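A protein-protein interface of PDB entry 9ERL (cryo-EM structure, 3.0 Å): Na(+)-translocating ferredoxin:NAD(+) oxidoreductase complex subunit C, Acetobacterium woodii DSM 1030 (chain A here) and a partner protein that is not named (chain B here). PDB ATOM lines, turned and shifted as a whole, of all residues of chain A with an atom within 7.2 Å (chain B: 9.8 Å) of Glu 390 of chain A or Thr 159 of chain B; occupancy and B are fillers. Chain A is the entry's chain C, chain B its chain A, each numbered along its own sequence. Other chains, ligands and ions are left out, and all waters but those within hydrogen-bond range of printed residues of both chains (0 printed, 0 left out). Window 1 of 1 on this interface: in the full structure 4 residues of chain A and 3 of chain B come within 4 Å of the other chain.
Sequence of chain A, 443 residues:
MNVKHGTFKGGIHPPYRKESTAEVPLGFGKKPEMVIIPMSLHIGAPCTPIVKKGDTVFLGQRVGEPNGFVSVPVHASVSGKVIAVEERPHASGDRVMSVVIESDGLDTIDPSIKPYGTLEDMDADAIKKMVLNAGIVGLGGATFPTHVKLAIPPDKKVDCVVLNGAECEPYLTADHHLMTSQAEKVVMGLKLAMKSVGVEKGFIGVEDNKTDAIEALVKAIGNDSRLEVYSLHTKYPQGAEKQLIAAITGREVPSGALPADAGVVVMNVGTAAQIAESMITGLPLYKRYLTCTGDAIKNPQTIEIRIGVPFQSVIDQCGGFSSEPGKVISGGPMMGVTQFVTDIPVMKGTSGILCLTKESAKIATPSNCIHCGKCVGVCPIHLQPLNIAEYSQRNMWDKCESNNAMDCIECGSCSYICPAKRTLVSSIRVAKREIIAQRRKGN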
ATOM      1  N   SER A 367       5.087 -12.748  -7.630  1.00  0.00           N
ATOM      2  CA  SER A 367       5.954 -12.180  -6.605  1.00  0.00           C
ATOM      3  C   SER A 367       5.912 -13.009  -5.328  1.00  0.00           C
ATOM      4  O   SER A 367       5.397 -14.132  -5.324  1.00  0.00           O
ATOM      5  CB  SER A 367       5.557 -10.735  -6.305  1.00  0.00           C
ATOM      6  OG  SER A 367       5.464  -9.972  -7.492  1.00  0.00           O
ATOM      7  N   ASN A 368       6.461 -12.467  -4.244  1.00  0.00           N
ATOM      8  CA  ASN A 368       6.486 -13.162  -2.965  1.00  0.00           C
ATOM      9  C   ASN A 368       5.101 -13.196  -2.326  1.00  0.00           C
ATOM     10  O   ASN A 368       4.264 -12.319  -2.552  1.00  0.00           O
ATOM     11  CB  ASN A 368       7.472 -12.487  -2.014  1.00  0.00           C
ATOM     12  CG  ASN A 368       8.824 -13.166  -1.996  1.00  0.00           C
ATOM     13  OD1 ASN A 368       9.091 -14.067  -2.789  1.00  0.00           O
ATOM     14  ND2 ASN A 368       9.688 -12.736  -1.086  1.00  0.00           N
ATOM     15  N   CYS A 369       4.867 -14.227  -1.517  1.00  0.00           N
ATOM     16  CA  CYS A 369       3.635 -14.335  -0.748  1.00  0.00           C
ATOM     17  C   CYS A 369       3.672 -13.380   0.438  1.00  0.00           C
ATOM     18  O   CYS A 369       4.698 -13.243   1.109  1.00  0.00           O
ATOM     19  CB  CYS A 369       3.436 -15.771  -0.264  1.00  0.00           C
ATOM     20  SG  CYS A 369       1.830 -16.117   0.485  1.00  0.00           S
ATOM     21  N   HIS A 371       1.061 -13.416   2.850  1.00  0.00           N
ATOM     22  CA  HIS A 371       0.265 -14.019   3.926  1.00  0.00           C
ATOM     23  C   HIS A 371      -1.020 -13.244   4.210  1.00  0.00           C
ATOM     24  O   HIS A 371      -1.413 -13.065   5.364  1.00  0.00           O
ATOM     25  CB  HIS A 371       1.092 -14.170   5.204  1.00  0.00           C
ATOM     26  CG  HIS A 371       1.779 -15.492   5.328  1.00  0.00           C
ATOM     27  ND1 HIS A 371       1.322 -16.493   6.156  1.00  0.00           N
ATOM     28  CD2 HIS A 371       2.891 -15.978   4.728  1.00  0.00           C
ATOM     29  CE1 HIS A 371       2.121 -17.539   6.060  1.00  0.00           C
ATOM     30  NE2 HIS A 371       3.081 -17.253   5.200  1.00  0.00           N
ATOM     31  N   PRO A 385      -4.748 -23.208   0.078  1.00  0.00           N
ATOM     32  CA  PRO A 385      -3.950 -23.322  -1.159  1.00  0.00           C
ATOM     33  C   PRO A 385      -2.492 -22.913  -1.024  1.00  0.00           C
ATOM     34  O   PRO A 385      -1.645 -23.451  -1.751  1.00  0.00           O
ATOM     35  CB  PRO A 385      -4.699 -22.403  -2.134  1.00  0.00           C
ATOM     36  CG  PRO A 385      -6.082 -22.307  -1.583  1.00  0.00           C
ATOM     37  CD  PRO A 385      -5.930 -22.352  -0.102  1.00  0.00           C
ATOM     38  N   LEU A 386      -2.175 -21.968  -0.133  1.00  0.00           N
ATOM     39  CA  LEU A 386      -0.804 -21.473  -0.036  1.00  0.00           C
ATOM     40  C   LEU A 386       0.156 -22.568   0.415  1.00  0.00           C
ATOM     41  O   LEU A 386       1.255 -22.703  -0.136  1.00  0.00           O
ATOM     42  CB  LEU A 386      -0.743 -20.265   0.905  1.00  0.00           C
ATOM     43  CG  LEU A 386      -1.023 -20.373   2.408  1.00  0.00           C
ATOM     44  CD1 LEU A 386      -0.262 -19.304   3.168  1.00  0.00           C
ATOM     45  CD2 LEU A 386      -2.506 -20.265   2.705  1.00  0.00           C
ATOM     46  N   ASN A 387      -0.250 -23.378   1.396  1.00  0.00           N
ATOM     47  CA  ASN A 387       0.622 -24.440   1.888  1.00  0.00           C
ATOM     48  C   ASN A 387       0.842 -25.516   0.831  1.00  0.00           C
ATOM     49  O   ASN A 387       1.968 -25.997   0.658  1.00  0.00           O
ATOM     50  CB  ASN A 387       0.036 -25.046   3.161  1.00  0.00           C
ATOM     51  CG  ASN A 387       0.052 -24.078   4.325  1.00  0.00           C
ATOM     52  OD1 ASN A 387       1.027 -23.362   4.537  1.00  0.00           O
ATOM     53  ND2 ASN A 387      -1.035 -24.050   5.084  1.00  0.00           N
ATOM     54  N   ILE A 388      -0.217 -25.897   0.111  1.00  0.00           N
ATOM     55  CA  ILE A 388      -0.080 -26.902  -0.942  1.00  0.00           C
ATOM     56  C   ILE A 388       0.836 -26.395  -2.047  1.00  0.00           C
ATOM     57  O   ILE A 388       1.688 -27.135  -2.552  1.00  0.00           O
ATOM     58  CB  ILE A 388      -1.461 -27.303  -1.495  1.00  0.00           C
ATOM     59  CG1 ILE A 388      -2.377 -27.790  -0.375  1.00  0.00           C
ATOM     60  CG2 ILE A 388      -1.317 -28.385  -2.550  1.00  0.00           C
ATOM     61  CD1 ILE A 388      -3.842 -27.767  -0.745  1.00  0.00           C
ATOM     62  N   ALA A 389       0.680 -25.126  -2.439  1.00  0.00           N
ATOM     63  CA  ALA A 389       1.538 -24.566  -3.481  1.00  0.00           C
ATOM     64  C   ALA A 389       2.997 -24.510  -3.039  1.00  0.00           C
ATOM     65  O   ALA A 389       3.900 -24.861  -3.810  1.00  0.00           O
ATOM     66  CB  ALA A 389       1.042 -23.178  -3.879  1.00  0.00           C
ATOM     67  N   GLU A 390       3.250 -24.083  -1.796  1.00  0.00           N
ATOM     68  CA  GLU A 390       4.627 -23.999  -1.318  1.00  0.00           C
ATOM     69  C   GLU A 390       5.262 -25.375  -1.167  1.00  0.00           C
ATOM     70  O   GLU A 390       6.467 -25.525  -1.397  1.00  0.00           O
ATOM     71  CB  GLU A 390       4.688 -23.242   0.009  1.00  0.00           C
ATOM     72  CG  GLU A 390       4.279 -21.779  -0.084  1.00  0.00           C
ATOM     73  CD  GLU A 390       5.367 -20.896  -0.656  1.00  0.00           C
ATOM     74  OE1 GLU A 390       6.518 -20.982  -0.181  1.00  0.00           O
ATOM     75  OE2 GLU A 390       5.069 -20.114  -1.581  1.00  0.00           O
ATOM     76  N   TYR A 391       4.484 -26.386  -0.772  1.00  0.00           N
ATOM     77  CA  TYR A 391       5.025 -27.740  -0.695  1.00  0.00           C
ATOM     78  C   TYR A 391       5.283 -28.314  -2.082  1.00  0.00           C
ATOM     79  O   TYR A 391       6.271 -29.027  -2.289  1.00  0.00           O
ATOM     80  CB  TYR A 391       4.074 -28.643   0.089  1.00  0.00           C
ATOM     81  CG  TYR A 391       4.122 -28.441   1.584  1.00  0.00           C
ATOM     82  CD1 TYR A 391       5.326 -28.227   2.236  1.00  0.00           C
ATOM     83  CD2 TYR A 391       2.961 -28.456   2.342  1.00  0.00           C
ATOM     84  CE1 TYR A 391       5.374 -28.041   3.600  1.00  0.00           C
ATOM     85  CE2 TYR A 391       2.999 -28.268   3.706  1.00  0.00           C
ATOM     86  CZ  TYR A 391       4.208 -28.061   4.330  1.00  0.00           C
ATOM     87  OH  TYR A 391       4.251 -27.874   5.692  1.00  0.00           O
ATOM     88  N   SER A 392       4.406 -28.018  -3.044  1.00  0.00           N
ATOM     89  CA  SER A 392       4.573 -28.547  -4.392  1.00  0.00           C
ATOM     90  C   SER A 392       5.734 -27.890  -5.121  1.00  0.00           C
ATOM     91  O   SER A 392       6.349 -28.517  -5.991  1.00  0.00           O
ATOM     92  CB  SER A 392       3.285 -28.361  -5.191  1.00  0.00           C
ATOM     93  OG  SER A 392       3.498 -28.615  -6.566  1.00  0.00           O
ATOM     94  N   GLN A 393       6.047 -26.635  -4.794  1.00  0.00           N
ATOM     95  CA  GLN A 393       7.110 -25.934  -5.504  1.00  0.00           C
ATOM     96  C   GLN A 393       8.505 -26.454  -5.175  1.00  0.00           C
ATOM     97  O   GLN A 393       9.449 -26.123  -5.900  1.00  0.00           O
ATOM     98  CB  GLN A 393       7.034 -24.439  -5.206  1.00  0.00           C
ATOM     99  CG  GLN A 393       6.005 -23.709  -6.043  1.00  0.00           C
ATOM    100  CD  GLN A 393       6.392 -22.274  -6.318  1.00  0.00           C
ATOM    101  OE1 GLN A 393       6.521 -21.468  -5.399  1.00  0.00           O
ATOM    102  NE2 GLN A 393       6.583 -21.947  -7.590  1.00  0.00           N
ATOM    103  N   ARG A 394       8.668 -27.250  -4.116  1.00  0.00           N
ATOM    104  CA  ARG A 394       9.974 -27.793  -3.754  1.00  0.00           C
ATOM    105  C   ARG A 394       9.970 -29.317  -3.683  1.00  0.00           C
ATOM    106  O   ARG A 394      10.795 -29.899  -2.971  1.00  0.00           O
ATOM    107  CB  ARG A 394      10.459 -27.199  -2.430  1.00  0.00           C
ATOM    108  CG  ARG A 394       9.397 -27.088  -1.360  1.00  0.00           C
ATOM    109  CD  ARG A 394       9.779 -26.057  -0.312  1.00  0.00           C
ATOM    110  NE  ARG A 394       9.415 -24.704  -0.714  1.00  0.00           N
ATOM    111  CZ  ARG A 394      10.035 -23.608  -0.304  1.00  0.00           C
ATOM    112  NH1 ARG A 394      11.072 -23.665   0.514  1.00  0.00           N
ATOM    113  NH2 ARG A 394       9.604 -22.422  -0.726  1.00  0.00           N
ATOM    114  N   ASN A 395       9.051 -29.966  -4.402  1.00  0.00           N
ATOM    115  CA  ASN A 395       9.025 -31.419  -4.596  1.00  0.00           C
ATOM    116  C   ASN A 395       8.891 -32.173  -3.270  1.00  0.00           C
ATOM    117  O   ASN A 395       9.740 -32.982  -2.893  1.00  0.00           O
ATOM    118  CB  ASN A 395      10.260 -31.888  -5.374  1.00  0.00           C
ATOM    119  CG  ASN A 395      10.427 -31.163  -6.693  1.00  0.00           C
ATOM    120  OD1 ASN A 395       9.451 -30.740  -7.309  1.00  0.00           O
ATOM    121  ND2 ASN A 395      11.670 -31.017  -7.135  1.00  0.00           N
ATOM    122  N   MET A 396       7.794 -31.901  -2.569  1.00  0.00           N
ATOM    123  CA  MET A 396       7.436 -32.601  -1.337  1.00  0.00           C
ATOM    124  C   MET A 396       6.027 -33.154  -1.527  1.00  0.00           C
ATOM    125  O   MET A 396       5.045 -32.526  -1.126  1.00  0.00           O
ATOM    126  CB  MET A 396       7.519 -31.671  -0.127  1.00  0.00           C
ATOM    127  CG  MET A 396       8.933 -31.288   0.275  1.00  0.00           C
ATOM    128  SD  MET A 396       9.009 -29.704   1.133  1.00  0.00           S
ATOM    129  CE  MET A 396       9.351 -30.233   2.806  1.00  0.00           C
ATOM    130  N   CYS A 400       2.115 -32.655   0.384  1.00  0.00           N
ATOM    131  CA  CYS A 400       0.964 -32.277  -0.431  1.00  0.00           C
ATOM    132  C   CYS A 400      -0.186 -33.258  -0.246  1.00  0.00           C
ATOM    133  O   CYS A 400      -1.347 -32.850  -0.136  1.00  0.00           O
ATOM    134  CB  CYS A 400       1.364 -32.197  -1.903  1.00  0.00           C
ATOM    135  SG  CYS A 400       2.486 -30.851  -2.312  1.00  0.00           S
ATOM    136  N   ARG A 422       0.036 -15.186  -8.308  1.00  0.00           N
ATOM    137  CA  ARG A 422       0.727 -16.465  -8.345  1.00  0.00           C
ATOM    138  C   ARG A 422      -0.063 -17.478  -9.172  1.00  0.00           C
ATOM    139  O   ARG A 422      -1.090 -17.164  -9.778  1.00  0.00           O
ATOM    140  CB  ARG A 422       0.975 -16.973  -6.927  1.00  0.00           C
ATOM    141  CG  ARG A 422       1.473 -15.900  -5.979  1.00  0.00           C
ATOM    142  CD  ARG A 422       2.099 -16.492  -4.733  1.00  0.00           C
ATOM    143  NE  ARG A 422       3.519 -16.755  -4.917  1.00  0.00           N
ATOM    144  CZ  ARG A 422       4.135 -17.850  -4.497  1.00  0.00           C
ATOM    145  NH1 ARG A 422       3.487 -18.804  -3.849  1.00  0.00           N
ATOM    146  NH2 ARG A 422       5.437 -17.992  -4.734  1.00  0.00           N
ATOM    147  N   LEU A 424      -1.265 -20.811  -8.206  1.00  0.00           N
ATOM    148  CA  LEU A 424      -1.531 -21.849  -7.212  1.00  0.00           C
ATOM    149  C   LEU A 424      -2.191 -23.082  -7.824  1.00  0.00           C
ATOM    150  O   LEU A 424      -1.832 -24.219  -7.485  1.00  0.00           O
ATOM    151  CB  LEU A 424      -2.403 -21.275  -6.095  1.00  0.00           C
ATOM    152  CG  LEU A 424      -2.017 -19.878  -5.603  1.00  0.00           C
ATOM    153  CD1 LEU A 424      -3.066 -19.330  -4.659  1.00  0.00           C
ATOM    154  CD2 LEU A 424      -0.665 -19.915  -4.925  1.00  0.00           C
ATOM    155  N   SER A 427       0.237 -25.412  -9.615  1.00  0.00           N
ATOM    156  CA  SER A 427       1.028 -26.201  -8.675  1.00  0.00           C
ATOM    157  C   SER A 427       0.203 -27.334  -8.076  1.00  0.00           C
ATOM    158  O   SER A 427       0.708 -28.450  -7.885  1.00  0.00           O
ATOM    159  CB  SER A 427       1.580 -25.297  -7.575  1.00  0.00           C
ATOM    160  OG  SER A 427       2.359 -24.250  -8.123  1.00  0.00           O
ATOM    161  N   GLY B 152       7.657 -25.854  16.876  1.00  0.00           N
ATOM    162  CA  GLY B 152       6.596 -25.278  16.062  1.00  0.00           C
ATOM    163  C   GLY B 152       7.089 -24.176  15.143  1.00  0.00           C
ATOM    164  O   GLY B 152       6.698 -24.105  13.971  1.00  0.00           O
ATOM    165  N   ILE B 153       7.967 -23.306  15.654  1.00  0.00           N
ATOM    166  CA  ILE B 153       8.499 -22.222  14.828  1.00  0.00           C
ATOM    167  C   ILE B 153       9.341 -22.778  13.684  1.00  0.00           C
ATOM    168  O   ILE B 153       9.278 -22.283  12.552  1.00  0.00           O
ATOM    169  CB  ILE B 153       9.295 -21.226  15.691  1.00  0.00           C
ATOM    170  CG1 ILE B 153       8.360 -20.457  16.623  1.00  0.00           C
ATOM    171  CG2 ILE B 153      10.053 -20.245  14.822  1.00  0.00           C
ATOM    172  CD1 ILE B 153       9.049 -19.895  17.836  1.00  0.00           C
ATOM    173  N   ARG B 154      10.140 -23.816  13.954  1.00  0.00           N
ATOM    174  CA  ARG B 154      10.944 -24.419  12.891  1.00  0.00           C
ATOM    175  C   ARG B 154      10.068 -25.075  11.825  1.00  0.00           C
ATOM    176  O   ARG B 154      10.349 -24.964  10.621  1.00  0.00           O
ATOM    177  CB  ARG B 154      11.922 -25.428  13.487  1.00  0.00           C
ATOM    178  CG  ARG B 154      13.076 -24.789  14.240  1.00  0.00           C
ATOM    179  CD  ARG B 154      14.070 -25.833  14.716  1.00  0.00           C
ATOM    180  NE  ARG B 154      15.153 -26.033  13.761  1.00  0.00           N
ATOM    181  CZ  ARG B 154      16.258 -26.721  14.017  1.00  0.00           C
ATOM    182  NH1 ARG B 154      16.461 -27.291  15.192  1.00  0.00           N
ATOM    183  NH2 ARG B 154      17.180 -26.842  13.067  1.00  0.00           N
ATOM    184  N   GLU B 155       8.999 -25.759  12.246  1.00  0.00           N
ATOM    185  CA  GLU B 155       8.076 -26.348  11.280  1.00  0.00           C
ATOM    186  C   GLU B 155       7.407 -25.275  10.428  1.00  0.00           C
ATOM    187  O   GLU B 155       7.150 -25.490   9.238  1.00  0.00           O
ATOM    188  CB  GLU B 155       7.026 -27.192  11.999  1.00  0.00           C
ATOM    189  CG  GLU B 155       7.563 -28.483  12.586  1.00  0.00           C
ATOM    190  CD  GLU B 155       6.522 -29.583  12.616  1.00  0.00           C
ATOM    191  OE1 GLU B 155       5.456 -29.374  13.230  1.00  0.00           O
ATOM    192  OE2 GLU B 155       6.769 -30.656  12.029  1.00  0.00           O
ATOM    193  N   ARG B 156       7.104 -24.116  11.023  1.00  0.00           N
ATOM    194  CA  ARG B 156       6.598 -22.995  10.232  1.00  0.00           C
ATOM    195  C   ARG B 156       7.645 -22.491   9.242  1.00  0.00           C
ATOM    196  O   ARG B 156       7.331 -22.231   8.074  1.00  0.00           O
ATOM    197  CB  ARG B 156       6.139 -21.865  11.156  1.00  0.00           C
ATOM    198  CG  ARG B 156       6.303 -20.457  10.588  1.00  0.00           C
ATOM    199  CD  ARG B 156       5.184 -20.088   9.627  1.00  0.00           C
ATOM    200  NE  ARG B 156       5.589 -19.039   8.699  1.00  0.00           N
ATOM    201  CZ  ARG B 156       5.277 -17.757   8.833  1.00  0.00           C
ATOM    202  NH1 ARG B 156       4.545 -17.327   9.847  1.00  0.00           N
ATOM    203  NH2 ARG B 156       5.706 -16.886   7.927  1.00  0.00           N
ATOM    204  N   LEU B 157       8.898 -22.361   9.686  1.00  0.00           N
ATOM    205  CA  LEU B 157       9.969 -21.848   8.834  1.00  0.00           C
ATOM    206  C   LEU B 157      10.381 -22.823   7.743  1.00  0.00           C
ATOM    207  O   LEU B 157      11.170 -22.448   6.871  1.00  0.00           O
ATOM    208  CB  LEU B 157      11.198 -21.496   9.672  1.00  0.00           C
ATOM    209  CG  LEU B 157      11.237 -20.137  10.368  1.00  0.00           C
ATOM    210  CD1 LEU B 157      12.620 -19.900  10.942  1.00  0.00           C
ATOM    211  CD2 LEU B 157      10.848 -19.024   9.410  1.00  0.00           C
ATOM    212  N   GLU B 158       9.892 -24.065   7.792  1.00  0.00           N
ATOM    213  CA  GLU B 158      10.202 -25.037   6.743  1.00  0.00           C
ATOM    214  C   GLU B 158       9.765 -24.587   5.349  1.00  0.00           C
ATOM    215  O   GLU B 158      10.288 -25.108   4.358  1.00  0.00           O
ATOM    216  CB  GLU B 158       9.548 -26.381   7.070  1.00  0.00           C
ATOM    217  CG  GLU B 158      10.529 -27.525   7.246  1.00  0.00           C
ATOM    218  CD  GLU B 158       9.844 -28.820   7.630  1.00  0.00           C
ATOM    219  OE1 GLU B 158       8.678 -29.018   7.230  1.00  0.00           O
ATOM    220  OE2 GLU B 158      10.468 -29.639   8.337  1.00  0.00           O
ATOM    221  N   THR B 159       8.824 -23.649   5.240  1.00  0.00           N
ATOM    222  CA  THR B 159       8.362 -23.130   3.953  1.00  0.00           C
ATOM    223  C   THR B 159       8.805 -21.686   3.720  1.00  0.00           C
ATOM    224  O   THR B 159       8.067 -20.882   3.150  1.00  0.00           O
ATOM    225  CB  THR B 159       6.843 -23.226   3.834  1.00  0.00           C
ATOM    226  OG1 THR B 159       6.232 -22.709   5.022  1.00  0.00           O
ATOM    227  CG2 THR B 159       6.414 -24.660   3.633  1.00  0.00           C
ATOM    228  N   SER B 160      10.014 -21.343   4.150  1.00  0.00           N
ATOM    229  CA  SER B 160      10.574 -20.017   3.939  1.00  0.00           C
ATOM    230  C   SER B 160      11.847 -20.126   3.112  1.00  0.00           C
ATOM    231  O   SER B 160      12.490 -21.177   3.057  1.00  0.00           O
ATOM    232  CB  SER B 160      10.867 -19.311   5.268  1.00  0.00           C
ATOM    233  OG  SER B 160       9.684 -18.784   5.838  1.00  0.00           O
ATOM    234  N   ALA B 161      12.207 -19.022   2.467  1.00  0.00           N
ATOM    235  CA  ALA B 161      13.327 -19.001   1.527  1.00  0.00           C
ATOM    236  C   ALA B 161      14.605 -18.494   2.197  1.00  0.00           C
ATOM    237  O   ALA B 161      15.133 -17.435   1.865  1.00  0.00           O
ATOM    238  CB  ALA B 161      12.971 -18.157   0.308  1.00  0.00           C
ATOM    239  N   VAL B 162      15.107 -19.276   3.149  1.00  0.00           N
ATOM    240  CA  VAL B 162      16.424 -19.030   3.737  1.00  0.00           C
ATOM    241  C   VAL B 162      17.435 -19.294   2.628  1.00  0.00           C
ATOM    242  O   VAL B 162      17.452 -20.404   2.076  1.00  0.00           O
ATOM    243  CB  VAL B 162      16.658 -19.914   4.971  1.00  0.00           C
ATOM    244  CG1 VAL B 162      17.834 -19.405   5.777  1.00  0.00           C
ATOM    245  CG2 VAL B 162      15.406 -19.957   5.829  1.00  0.00           C
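O of Tyr 391 of chain A lies within hydrogen-bond range of N of Met 396 of chain A (3.3 Å).
NH2 of Arg 394 of chain A lies within salt-bridge range of OE1 of Glu 390 of chain A (3.4 Å).
O of Arg 156 of chain B is in hydrogen-bond range of OG1 of Thr 159 of chain B (3.3 Å).
The backbone NH (N) of His 371 of chain A sits close to the side-chain sulfur (SG) of Cys 369 of chain A, 3.7 Å away.
NH1 of Arg 422 of chain A lies within salt-bridge range of OE2 of Glu 390 of chain A, 3.1 Å away.
His 371 of chain A touches Arg 156 of chain B (NE2 to NH2, 3.8 Å).
Glu 390 of chain A touches Thr 159 of chain B.
Thr 159 of chain B touches Tyr 391 of chain A (CG2 to CE1, 3.5 Å).
Arg 394 of chain A touches Ser 160 of chain B (NH1 to O, 3.8 Å).
Of the printed residues of chain B, His 371 of chain A touches Arg 156 (3.8 Å).
Of the printed residues of chain B, Glu 390 of chain A touches Thr 159 (3.7 Å).
Of the printed residues of chain B, Arg 394 of chain A touches Ser 160 (3.8 Å).
Met 396 of chain A touches none of the printed residues of chain B.
Printed residues of chain A within 4 Å of Arg 156 of chain B: His 371 (3.8 Å).
Of chain A, only Glu 390 and Tyr 391 come within 4 Å of Thr 159 of chain B.
Of the printed residues of chain A, Ser 160 of chain B touches Arg 394 (3.8 Å).
The nearest residue of chain A that does not touch Thr 159 of chain B is Arg 394 of chain A (4.4 Å).
The nearest printed residue of chain A that does not touch Arg 156 of chain B is Tyr 391 of chain A (6.9 Å).
Printed residues of chain A that touch a printed residue of chain B: His 371, Glu 390, Tyr 391 and Arg 394.
Hydrophobic or aromatic side chains of chain A that line the printed part of chain B: His 371 and Tyr 391.
Printed residues of chain B that touch a printed residue of chain A: Arg 156, Thr 159 and Ser 160.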
